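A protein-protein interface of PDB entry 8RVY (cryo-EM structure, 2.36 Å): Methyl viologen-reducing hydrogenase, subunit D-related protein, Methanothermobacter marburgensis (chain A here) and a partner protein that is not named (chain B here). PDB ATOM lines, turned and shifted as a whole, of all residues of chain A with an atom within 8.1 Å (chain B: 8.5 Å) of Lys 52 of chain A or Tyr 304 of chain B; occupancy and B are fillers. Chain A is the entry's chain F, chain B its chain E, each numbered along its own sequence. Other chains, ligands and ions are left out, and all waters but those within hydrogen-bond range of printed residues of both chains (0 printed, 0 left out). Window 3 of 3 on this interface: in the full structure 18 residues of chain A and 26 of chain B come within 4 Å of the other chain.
The backbone NH of Leu 316 of chain B sits close to the side-chain carboxylate of Asp 314 of chain B (3.1 Å). The side-chain carboxylate of Glu 299 of chain B lies within hydrogen-bond range of a ring nitrogen (NE2) of His 325 of chain B, 3.3 Å away. The backbone NH (N) of Ser 48 of chain A sits close to the side-chain amide oxygen (OD1) of Asn 46 of chain A, at 3.4 Å. The side-chain hydroxyl (OG) of Ser 55 of chain A sits at hydrogen-bond distance from the backbone carbonyl oxygen (O) of Lys 52 of chain A (3.4 Å). The backbone carbonyl oxygen of Asp 314 of chain B is in hydrogen-bond range of the side-chain hydroxyl of Thr 317 of chain B, 3.5 Å away. The backbone carbonyl oxygen (O) of Leu 316 of chain B sits at hydrogen-bond distance from the backbone NH (N) of Val 321 of chain B, at 3.3 Å.
Ala 47 of chain A touches none of the printed residues of chain B. Printed residues of chain B within 4 Å of Ser 48 of chain A: Glu 299 (3.3 Å) and Val 321 (3.8 Å). No residue of chain B comes within 4 Å of Ala 53 of chain A. Printed residues of chain B within 4 Å of Ser 55 of chain A: Asp 314, Leu 316 and Thr 317. Printed residues of chain A within 4 Å of Glu 299 of chain B: Ser 48 (3.3 Å). Leu 306 of chain B touches none of the printed residues of chain A. Of the printed residues of chain A, Asp 314 of chain B touches Ser 55 (3.5 Å). Printed residues of chain A within 4 Å of Thr 317 of chain B: Ser 55 (3.9 Å). The nearest residue of chain B that does not touch Lys 52 of chain A is Thr 317 of chain B (4.5 Å). The nearest residue of chain A that does not touch Tyr 304 of chain B is Glu 56 of chain A (5.5 Å).
Printed residues of chain A that touch a printed residue of chain B: Ser 48, Leu 51, Lys 52 and Ser 55. Hydrophobic or aromatic side chains of chain A within 4 Å of the printed part of chain B: Leu 51. Along chain A the printed residues that touch a printed residue of chain B span positions 48 to 55. Hydrophobic or aromatic side chains of chain B within 4 Å of the printed part of chain A: Leu 316 and Val 321. Along chain B the printed residues that touch a printed residue of chain A span positions 299 to 321. Among the printed residues, 8 pairs touch across the chains.
The side-chain carboxylate (OE2) of Glu 299 of chain B lies within hydrogen-bond range of the side-chain hydroxyl (OG) of Ser 48 of chain A (3.3 Å). NZ of Lys 52 of chain A is in hydrogen-bond range of O of Tyr 304 of chain B (3.1 Å).
Among the printed residues, merely in contact across the chains: Ser 48 of chain A with Val 321 of chain B (3.8 Å), Leu 51 of chain A with Leu 316 of chain B (3.7 Å), Leu 51 of chain A with Val 321 of chain B (3.6 Å), Ser 55 of chain A with Asp 314 of chain B (3.5 Å), Ser 55 of chain A with Leu 316 of chain B (3.9 Å) and Ser 55 of chain A with Thr 317 of chain B (3.9 Å).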
ATOM      1  N   VAL A   8     -24.724  17.972 -31.173  1.00  0.00           N
ATOM      2  CA  VAL A   8     -23.749  17.284 -32.011  1.00  0.00           C
ATOM      3  C   VAL A   8     -24.304  15.906 -32.339  1.00  0.00           C
ATOM      4  O   VAL A   8     -24.756  15.184 -31.445  1.00  0.00           O
ATOM      5  CB  VAL A   8     -22.381  17.173 -31.314  1.00  0.00           C
ATOM      6  CG1 VAL A   8     -21.550  16.067 -31.941  1.00  0.00           C
ATOM      7  CG2 VAL A   8     -21.644  18.492 -31.388  1.00  0.00           C
ATOM      8  N   PHE A  10     -23.874  12.104 -34.464  1.00  0.00           N
ATOM      9  CA  PHE A  10     -23.077  11.096 -35.147  1.00  0.00           C
ATOM     10  C   PHE A  10     -24.025  10.205 -35.934  1.00  0.00           C
ATOM     11  O   PHE A  10     -24.978   9.662 -35.370  1.00  0.00           O
ATOM     12  CB  PHE A  10     -22.259  10.256 -34.162  1.00  0.00           C
ATOM     13  CG  PHE A  10     -21.329  11.058 -33.302  1.00  0.00           C
ATOM     14  CD1 PHE A  10     -21.779  11.653 -32.137  1.00  0.00           C
ATOM     15  CD2 PHE A  10     -20.001  11.211 -33.655  1.00  0.00           C
ATOM     16  CE1 PHE A  10     -20.927  12.389 -31.346  1.00  0.00           C
ATOM     17  CE2 PHE A  10     -19.145  11.944 -32.867  1.00  0.00           C
ATOM     18  CZ  PHE A  10     -19.608  12.533 -31.710  1.00  0.00           C
ATOM     19  N   ARG A  44     -18.383   2.578 -34.603  1.00  0.00           N
ATOM     20  CA  ARG A  44     -17.225   3.445 -34.443  1.00  0.00           C
ATOM     21  C   ARG A  44     -17.354   4.376 -33.246  1.00  0.00           C
ATOM     22  O   ARG A  44     -16.333   4.836 -32.726  1.00  0.00           O
ATOM     23  CB  ARG A  44     -17.021   4.266 -35.719  1.00  0.00           C
ATOM     24  CG  ARG A  44     -15.770   5.121 -35.738  1.00  0.00           C
ATOM     25  CD  ARG A  44     -14.527   4.285 -35.924  1.00  0.00           C
ATOM     26  NE  ARG A  44     -13.309   5.064 -35.753  1.00  0.00           N
ATOM     27  CZ  ARG A  44     -12.858   5.508 -34.589  1.00  0.00           C
ATOM     28  NH1 ARG A  44     -13.506   5.274 -33.462  1.00  0.00           N
ATOM     29  NH2 ARG A  44     -11.727   6.204 -34.555  1.00  0.00           N
ATOM     30  N   ASN A  46     -17.893   5.601 -29.459  1.00  0.00           N
ATOM     31  CA  ASN A  46     -17.676   5.119 -28.103  1.00  0.00           C
ATOM     32  C   ASN A  46     -17.993   6.243 -27.123  1.00  0.00           C
ATOM     33  O   ASN A  46     -18.421   7.333 -27.509  1.00  0.00           O
ATOM     34  CB  ASN A  46     -16.244   4.603 -27.913  1.00  0.00           C
ATOM     35  CG  ASN A  46     -15.196   5.631 -28.260  1.00  0.00           C
ATOM     36  OD1 ASN A  46     -15.502   6.798 -28.476  1.00  0.00           O
ATOM     37  ND2 ASN A  46     -13.947   5.203 -28.309  1.00  0.00           N
ATOM     38  N   ALA A  47     -17.786   5.963 -25.836  1.00  0.00           N
ATOM     39  CA  ALA A  47     -18.117   6.940 -24.804  1.00  0.00           C
ATOM     40  C   ALA A  47     -17.201   8.151 -24.851  1.00  0.00           C
ATOM     41  O   ALA A  47     -17.612   9.244 -24.455  1.00  0.00           O
ATOM     42  CB  ALA A  47     -18.048   6.290 -23.426  1.00  0.00           C
ATOM     43  N   SER A  48     -15.964   7.983 -25.321  1.00  0.00           N
ATOM     44  CA  SER A  48     -15.044   9.111 -25.385  1.00  0.00           C
ATOM     45  C   SER A  48     -15.597  10.223 -26.264  1.00  0.00           C
ATOM     46  O   SER A  48     -15.497  11.403 -25.917  1.00  0.00           O
ATOM     47  CB  SER A  48     -13.683   8.651 -25.901  1.00  0.00           C
ATOM     48  OG  SER A  48     -12.988   7.917 -24.915  1.00  0.00           O
ATOM     49  N   MET A  49     -16.192   9.867 -27.403  1.00  0.00           N
ATOM     50  CA  MET A  49     -16.768  10.873 -28.288  1.00  0.00           C
ATOM     51  C   MET A  49     -17.903  11.625 -27.605  1.00  0.00           C
ATOM     52  O   MET A  49     -17.976  12.856 -27.672  1.00  0.00           O
ATOM     53  CB  MET A  49     -17.270  10.212 -29.571  1.00  0.00           C
ATOM     54  CG  MET A  49     -16.209  10.027 -30.630  1.00  0.00           C
ATOM     55  SD  MET A  49     -16.480   8.562 -31.637  1.00  0.00           S
ATOM     56  CE  MET A  49     -14.813   7.934 -31.764  1.00  0.00           C
ATOM     57  N   ILE A  50     -18.802  10.897 -26.944  1.00  0.00           N
ATOM     58  CA  ILE A  50     -19.949  11.538 -26.305  1.00  0.00           C
ATOM     59  C   ILE A  50     -19.484  12.452 -25.181  1.00  0.00           C
ATOM     60  O   ILE A  50     -19.962  13.584 -25.037  1.00  0.00           O
ATOM     61  CB  ILE A  50     -20.940  10.474 -25.792  1.00  0.00           C
ATOM     62  CG1 ILE A  50     -21.230   9.419 -26.864  1.00  0.00           C
ATOM     63  CG2 ILE A  50     -22.235  11.122 -25.337  1.00  0.00           C
ATOM     64  CD1 ILE A  50     -21.729   9.980 -28.167  1.00  0.00           C
ATOM     65  N   LEU A  51     -18.551  11.970 -24.360  1.00  0.00           N
ATOM     66  CA  LEU A  51     -18.055  12.767 -23.248  1.00  0.00           C
ATOM     67  C   LEU A  51     -17.310  13.998 -23.743  1.00  0.00           C
ATOM     68  O   LEU A  51     -17.430  15.076 -23.156  1.00  0.00           O
ATOM     69  CB  LEU A  51     -17.156  11.914 -22.356  1.00  0.00           C
ATOM     70  CG  LEU A  51     -17.840  10.709 -21.714  1.00  0.00           C
ATOM     71  CD1 LEU A  51     -16.815   9.735 -21.171  1.00  0.00           C
ATOM     72  CD2 LEU A  51     -18.788  11.157 -20.625  1.00  0.00           C
ATOM     73  N   LYS A  52     -16.531  13.857 -24.818  1.00  0.00           N
ATOM     74  CA  LYS A  52     -15.874  15.014 -25.409  1.00  0.00           C
ATOM     75  C   LYS A  52     -16.896  16.026 -25.902  1.00  0.00           C
ATOM     76  O   LYS A  52     -16.757  17.228 -25.656  1.00  0.00           O
ATOM     77  CB  LYS A  52     -14.967  14.562 -26.554  1.00  0.00           C
ATOM     78  CG  LYS A  52     -14.273  15.687 -27.308  1.00  0.00           C
ATOM     79  CD  LYS A  52     -13.051  16.177 -26.567  1.00  0.00           C
ATOM     80  CE  LYS A  52     -12.243  17.133 -27.417  1.00  0.00           C
ATOM     81  NZ  LYS A  52     -11.320  17.952 -26.592  1.00  0.00           N
ATOM     82  N   ALA A  53     -17.938  15.559 -26.588  1.00  0.00           N
ATOM     83  CA  ALA A  53     -18.953  16.476 -27.090  1.00  0.00           C
ATOM     84  C   ALA A  53     -19.627  17.226 -25.949  1.00  0.00           C
ATOM     85  O   ALA A  53     -19.853  18.437 -26.041  1.00  0.00           O
ATOM     86  CB  ALA A  53     -19.985  15.713 -27.917  1.00  0.00           C
ATOM     87  N   PHE A  54     -19.953  16.525 -24.864  1.00  0.00           N
ATOM     88  CA  PHE A  54     -20.594  17.194 -23.735  1.00  0.00           C
ATOM     89  C   PHE A  54     -19.640  18.159 -23.042  1.00  0.00           C
ATOM     90  O   PHE A  54     -20.056  19.232 -22.590  1.00  0.00           O
ATOM     91  CB  PHE A  54     -21.127  16.162 -22.743  1.00  0.00           C
ATOM     92  CG  PHE A  54     -22.492  15.642 -23.086  1.00  0.00           C
ATOM     93  CD1 PHE A  54     -23.549  16.511 -23.296  1.00  0.00           C
ATOM     94  CD2 PHE A  54     -22.719  14.286 -23.202  1.00  0.00           C
ATOM     95  CE1 PHE A  54     -24.795  16.036 -23.614  1.00  0.00           C
ATOM     96  CE2 PHE A  54     -23.965  13.809 -23.518  1.00  0.00           C
ATOM     97  CZ  PHE A  54     -25.006  14.685 -23.723  1.00  0.00           C
ATOM     98  N   SER A  55     -18.359  17.797 -22.941  1.00  0.00           N
ATOM     99  CA  SER A  55     -17.388  18.653 -22.271  1.00  0.00           C
ATOM    100  C   SER A  55     -16.991  19.854 -23.122  1.00  0.00           C
ATOM    101  O   SER A  55     -16.584  20.883 -22.573  1.00  0.00           O
ATOM    102  CB  SER A  55     -16.148  17.841 -21.899  1.00  0.00           C
ATOM    103  OG  SER A  55     -15.106  18.038 -22.833  1.00  0.00           O
ATOM    104  N   GLU A  56     -17.105  19.753 -24.444  1.00  0.00           N
ATOM    105  CA  GLU A  56     -16.803  20.872 -25.328  1.00  0.00           C
ATOM    106  C   GLU A  56     -17.962  21.849 -25.471  1.00  0.00           C
ATOM    107  O   GLU A  56     -17.810  22.853 -26.172  1.00  0.00           O
ATOM    108  CB  GLU A  56     -16.395  20.362 -26.713  1.00  0.00           C
ATOM    109  CG  GLU A  56     -15.070  19.630 -26.755  1.00  0.00           C
ATOM    110  CD  GLU A  56     -13.926  20.451 -26.199  1.00  0.00           C
ATOM    111  OE1 GLU A  56     -13.779  21.622 -26.605  1.00  0.00           O
ATOM    112  OE2 GLU A  56     -13.173  19.926 -25.353  1.00  0.00           O
ATOM    113  N   GLY A  57     -19.106  21.581 -24.848  1.00  0.00           N
ATOM    114  CA  GLY A  57     -20.177  22.556 -24.790  1.00  0.00           C
ATOM    115  C   GLY A  57     -21.466  22.145 -25.469  1.00  0.00           C
ATOM    116  O   GLY A  57     -22.342  22.984 -25.687  1.00  0.00           O
ATOM    117  N   ALA A  58     -21.605  20.867 -25.808  1.00  0.00           N
ATOM    118  CA  ALA A  58     -22.830  20.381 -26.427  1.00  0.00           C
ATOM    119  C   ALA A  58     -23.933  20.265 -25.384  1.00  0.00           C
ATOM    120  O   ALA A  58     -23.726  19.699 -24.308  1.00  0.00           O
ATOM    121  CB  ALA A  58     -22.594  19.030 -27.096  1.00  0.00           C
ATOM    122  N   VAL A  61     -26.514  15.374 -27.401  1.00  0.00           N
ATOM    123  CA  VAL A  61     -25.717  14.543 -28.292  1.00  0.00           C
ATOM    124  C   VAL A  61     -26.620  13.480 -28.895  1.00  0.00           C
ATOM    125  O   VAL A  61     -27.292  12.743 -28.166  1.00  0.00           O
ATOM    126  CB  VAL A  61     -24.527  13.891 -27.560  1.00  0.00           C
ATOM    127  CG1 VAL A  61     -23.808  12.924 -28.476  1.00  0.00           C
ATOM    128  CG2 VAL A  61     -23.570  14.950 -27.058  1.00  0.00           C
ATOM    129  N   CYS B 298      -1.864   5.318 -21.725  1.00  0.00           N
ATOM    130  CA  CYS B 298      -3.221   5.624 -21.308  1.00  0.00           C
ATOM    131  C   CYS B 298      -3.834   6.673 -22.224  1.00  0.00           C
ATOM    132  O   CYS B 298      -3.178   7.646 -22.605  1.00  0.00           O
ATOM    133  CB  CYS B 298      -3.242   6.116 -19.860  1.00  0.00           C
ATOM    134  SG  CYS B 298      -4.888   6.493 -19.232  1.00  0.00           S
ATOM    135  N   GLU B 299      -5.106   6.468 -22.570  1.00  0.00           N
ATOM    136  CA  GLU B 299      -5.812   7.427 -23.409  1.00  0.00           C
ATOM    137  C   GLU B 299      -6.023   8.757 -22.698  1.00  0.00           C
ATOM    138  O   GLU B 299      -6.132   9.797 -23.354  1.00  0.00           O
ATOM    139  CB  GLU B 299      -7.159   6.851 -23.840  1.00  0.00           C
ATOM    140  CG  GLU B 299      -7.574   7.240 -25.250  1.00  0.00           C
ATOM    141  CD  GLU B 299      -9.060   7.534 -25.375  1.00  0.00           C
ATOM    142  OE1 GLU B 299      -9.486   7.971 -26.465  1.00  0.00           O
ATOM    143  OE2 GLU B 299      -9.802   7.334 -24.392  1.00  0.00           O
ATOM    144  N   LEU B 300      -6.090   8.746 -21.366  1.00  0.00           N
ATOM    145  CA  LEU B 300      -6.352   9.972 -20.622  1.00  0.00           C
ATOM    146  C   LEU B 300      -5.241  10.997 -20.787  1.00  0.00           C
ATOM    147  O   LEU B 300      -5.452  12.175 -20.483  1.00  0.00           O
ATOM    148  CB  LEU B 300      -6.538   9.656 -19.141  1.00  0.00           C
ATOM    149  CG  LEU B 300      -7.664   8.688 -18.781  1.00  0.00           C
ATOM    150  CD1 LEU B 300      -7.711   8.478 -17.281  1.00  0.00           C
ATOM    151  CD2 LEU B 300      -8.999   9.186 -19.298  1.00  0.00           C
ATOM    152  N   GLU B 301      -4.066  10.579 -21.250  1.00  0.00           N
ATOM    153  CA  GLU B 301      -2.934  11.469 -21.449  1.00  0.00           C
ATOM    154  C   GLU B 301      -2.784  11.908 -22.899  1.00  0.00           C
ATOM    155  O   GLU B 301      -1.737  12.447 -23.266  1.00  0.00           O
ATOM    156  CB  GLU B 301      -1.651  10.791 -20.972  1.00  0.00           C
ATOM    157  CG  GLU B 301      -1.813  10.036 -19.673  1.00  0.00           C
ATOM    158  CD  GLU B 301      -0.497   9.564 -19.105  1.00  0.00           C
ATOM    159  OE1 GLU B 301       0.101   8.631 -19.681  1.00  0.00           O
ATOM    160  OE2 GLU B 301      -0.061  10.120 -18.079  1.00  0.00           O
ATOM    161  N   LYS B 302      -3.796  11.678 -23.728  1.00  0.00           N
ATOM    162  CA  LYS B 302      -3.779  12.149 -25.102  1.00  0.00           C
ATOM    163  C   LYS B 302      -4.118  13.634 -25.154  1.00  0.00           C
ATOM    164  O   LYS B 302      -4.758  14.187 -24.258  1.00  0.00           O
ATOM    165  CB  LYS B 302      -4.766  11.355 -25.952  1.00  0.00           C
ATOM    166  CG  LYS B 302      -4.389   9.903 -26.137  1.00  0.00           C
ATOM    167  CD  LYS B 302      -3.693   9.685 -27.461  1.00  0.00           C
ATOM    168  CE  LYS B 302      -3.221   8.250 -27.623  1.00  0.00           C
ATOM    169  NZ  LYS B 302      -4.237   7.255 -27.182  1.00  0.00           N
ATOM    170  N   ASP B 303      -3.690  14.279 -26.239  1.00  0.00           N
ATOM    171  CA  ASP B 303      -3.810  15.728 -26.327  1.00  0.00           C
ATOM    172  C   ASP B 303      -5.263  16.186 -26.299  1.00  0.00           C
ATOM    173  O   ASP B 303      -5.547  17.296 -25.840  1.00  0.00           O
ATOM    174  CB  ASP B 303      -3.114  16.235 -27.591  1.00  0.00           C
ATOM    175  CG  ASP B 303      -3.746  15.704 -28.861  1.00  0.00           C
ATOM    176  OD1 ASP B 303      -4.665  14.864 -28.771  1.00  0.00           O
ATOM    177  OD2 ASP B 303      -3.317  16.125 -29.956  1.00  0.00           O
ATOM    178  N   TYR B 304      -6.192  15.358 -26.774  1.00  0.00           N
ATOM    179  CA  TYR B 304      -7.596  15.746 -26.827  1.00  0.00           C
ATOM    180  C   TYR B 304      -8.361  15.413 -25.551  1.00  0.00           C
ATOM    181  O   TYR B 304      -9.545  15.746 -25.457  1.00  0.00           O
ATOM    182  CB  TYR B 304      -8.294  15.094 -28.030  1.00  0.00           C
ATOM    183  CG  TYR B 304      -8.071  13.608 -28.185  1.00  0.00           C
ATOM    184  CD1 TYR B 304      -8.828  12.693 -27.471  1.00  0.00           C
ATOM    185  CD2 TYR B 304      -7.116  13.121 -29.062  1.00  0.00           C
ATOM    186  CE1 TYR B 304      -8.631  11.338 -27.616  1.00  0.00           C
ATOM    187  CE2 TYR B 304      -6.911  11.769 -29.214  1.00  0.00           C
ATOM    188  CZ  TYR B 304      -7.671  10.882 -28.490  1.00  0.00           C
ATOM    189  OH  TYR B 304      -7.465   9.532 -28.645  1.00  0.00           O
ATOM    190  N   LEU B 305      -7.724  14.776 -24.574  1.00  0.00           N
ATOM    191  CA  LEU B 305      -8.335  14.511 -23.277  1.00  0.00           C
ATOM    192  C   LEU B 305      -7.604  15.181 -22.129  1.00  0.00           C
ATOM    193  O   LEU B 305      -8.246  15.712 -21.220  1.00  0.00           O
ATOM    194  CB  LEU B 305      -8.389  12.998 -23.013  1.00  0.00           C
ATOM    195  CG  LEU B 305      -9.449  12.180 -23.746  1.00  0.00           C
ATOM    196  CD1 LEU B 305      -9.407  10.743 -23.275  1.00  0.00           C
ATOM    197  CD2 LEU B 305     -10.835  12.759 -23.552  1.00  0.00           C
ATOM    198  N   LEU B 306      -6.276  15.180 -22.155  1.00  0.00           N
ATOM    199  CA  LEU B 306      -5.490  15.634 -21.019  1.00  0.00           C
ATOM    200  C   LEU B 306      -5.732  17.109 -20.730  1.00  0.00           C
ATOM    201  O   LEU B 306      -5.832  17.933 -21.641  1.00  0.00           O
ATOM    202  CB  LEU B 306      -4.007  15.386 -21.293  1.00  0.00           C
ATOM    203  CG  LEU B 306      -3.021  15.618 -20.150  1.00  0.00           C
ATOM    204  CD1 LEU B 306      -3.361  14.764 -18.943  1.00  0.00           C
ATOM    205  CD2 LEU B 306      -1.619  15.324 -20.635  1.00  0.00           C
ATOM    206  N   GLU B 307      -5.816  17.437 -19.444  1.00  0.00           N
ATOM    207  CA  GLU B 307      -5.923  18.822 -19.005  1.00  0.00           C
ATOM    208  C   GLU B 307      -4.561  19.499 -19.116  1.00  0.00           C
ATOM    209  O   GLU B 307      -3.613  19.114 -18.424  1.00  0.00           O
ATOM    210  CB  GLU B 307      -6.473  18.878 -17.581  1.00  0.00           C
ATOM    211  CG  GLU B 307      -6.393  20.240 -16.914  1.00  0.00           C
ATOM    212  CD  GLU B 307      -7.167  21.302 -17.661  1.00  0.00           C
ATOM    213  OE1 GLU B 307      -8.373  21.470 -17.381  1.00  0.00           O
ATOM    214  OE2 GLU B 307      -6.571  21.965 -18.532  1.00  0.00           O
ATOM    215  N   SER B 308      -4.461  20.493 -20.000  1.00  0.00           N
ATOM    216  CA  SER B 308      -3.188  21.174 -20.219  1.00  0.00           C
ATOM    217  C   SER B 308      -2.830  22.092 -19.055  1.00  0.00           C
ATOM    218  O   SER B 308      -1.689  22.082 -18.583  1.00  0.00           O
ATOM    219  CB  SER B 308      -3.238  21.957 -21.530  1.00  0.00           C
ATOM    220  OG  SER B 308      -2.028  22.657 -21.752  1.00  0.00           O
ATOM    221  N   ASP B 314     -11.638  18.513 -16.176  1.00  0.00           N
ATOM    222  CA  ASP B 314     -13.070  18.336 -16.346  1.00  0.00           C
ATOM    223  C   ASP B 314     -13.424  16.921 -15.911  1.00  0.00           C
ATOM    224  O   ASP B 314     -12.861  15.964 -16.457  1.00  0.00           O
ATOM    225  CB  ASP B 314     -13.469  18.569 -17.798  1.00  0.00           C
ATOM    226  CG  ASP B 314     -14.969  18.666 -17.985  1.00  0.00           C
ATOM    227  OD1 ASP B 314     -15.714  17.997 -17.245  1.00  0.00           O
ATOM    228  OD2 ASP B 314     -15.404  19.415 -18.881  1.00  0.00           O
ATOM    229  N   LEU B 316     -15.663  14.917 -16.635  1.00  0.00           N
ATOM    230  CA  LEU B 316     -16.067  14.055 -17.736  1.00  0.00           C
ATOM    231  C   LEU B 316     -14.857  13.387 -18.376  1.00  0.00           C
ATOM    232  O   LEU B 316     -14.671  12.181 -18.218  1.00  0.00           O
ATOM    233  CB  LEU B 316     -16.843  14.852 -18.783  1.00  0.00           C
ATOM    234  CG  LEU B 316     -18.263  15.252 -18.381  1.00  0.00           C
ATOM    235  CD1 LEU B 316     -18.803  16.308 -19.325  1.00  0.00           C
ATOM    236  CD2 LEU B 316     -19.174  14.044 -18.355  1.00  0.00           C
ATOM    237  N   THR B 317     -13.989  14.166 -19.015  1.00  0.00           N
ATOM    238  CA  THR B 317     -12.940  13.592 -19.847  1.00  0.00           C
ATOM    239  C   THR B 317     -11.907  12.795 -19.062  1.00  0.00           C
ATOM    240  O   THR B 317     -11.112  12.081 -19.679  1.00  0.00           O
ATOM    241  CB  THR B 317     -12.242  14.702 -20.631  1.00  0.00           C
ATOM    242  OG1 THR B 317     -12.250  15.909 -19.864  1.00  0.00           O
ATOM    243  CG2 THR B 317     -12.957  14.944 -21.947  1.00  0.00           C
ATOM    244  N   VAL B 321     -14.346   8.967 -18.723  1.00  0.00           N
ATOM    245  CA  VAL B 321     -13.626   8.159 -19.700  1.00  0.00           C
ATOM    246  C   VAL B 321     -13.060   6.908 -19.038  1.00  0.00           C
ATOM    247  O   VAL B 321     -13.197   5.798 -19.565  1.00  0.00           O
ATOM    248  CB  VAL B 321     -12.525   8.988 -20.385  1.00  0.00           C
ATOM    249  CG1 VAL B 321     -11.696   8.115 -21.305  1.00  0.00           C
ATOM    250  CG2 VAL B 321     -13.136  10.128 -21.165  1.00  0.00           C
ATOM    251  N   HIS B 325     -14.152   3.041 -19.728  1.00  0.00           N
ATOM    252  CA  HIS B 325     -13.113   2.076 -20.068  1.00  0.00           C
ATOM    253  C   HIS B 325     -13.179   0.819 -19.209  1.00  0.00           C
ATOM    254  O   HIS B 325     -13.005  -0.287 -19.728  1.00  0.00           O
ATOM    255  CB  HIS B 325     -11.737   2.718 -19.929  1.00  0.00           C
ATOM    256  CG  HIS B 325     -11.317   3.511 -21.123  1.00  0.00           C
ATOM    257  ND1 HIS B 325      -9.995   3.743 -21.432  1.00  0.00           N
ATOM    258  CD2 HIS B 325     -12.043   4.132 -22.080  1.00  0.00           C
ATOM    259  CE1 HIS B 325      -9.926   4.470 -22.532  1.00  0.00           C
ATOM    260  NE2 HIS B 325     -11.154   4.721 -22.943  1.00  0.00           N
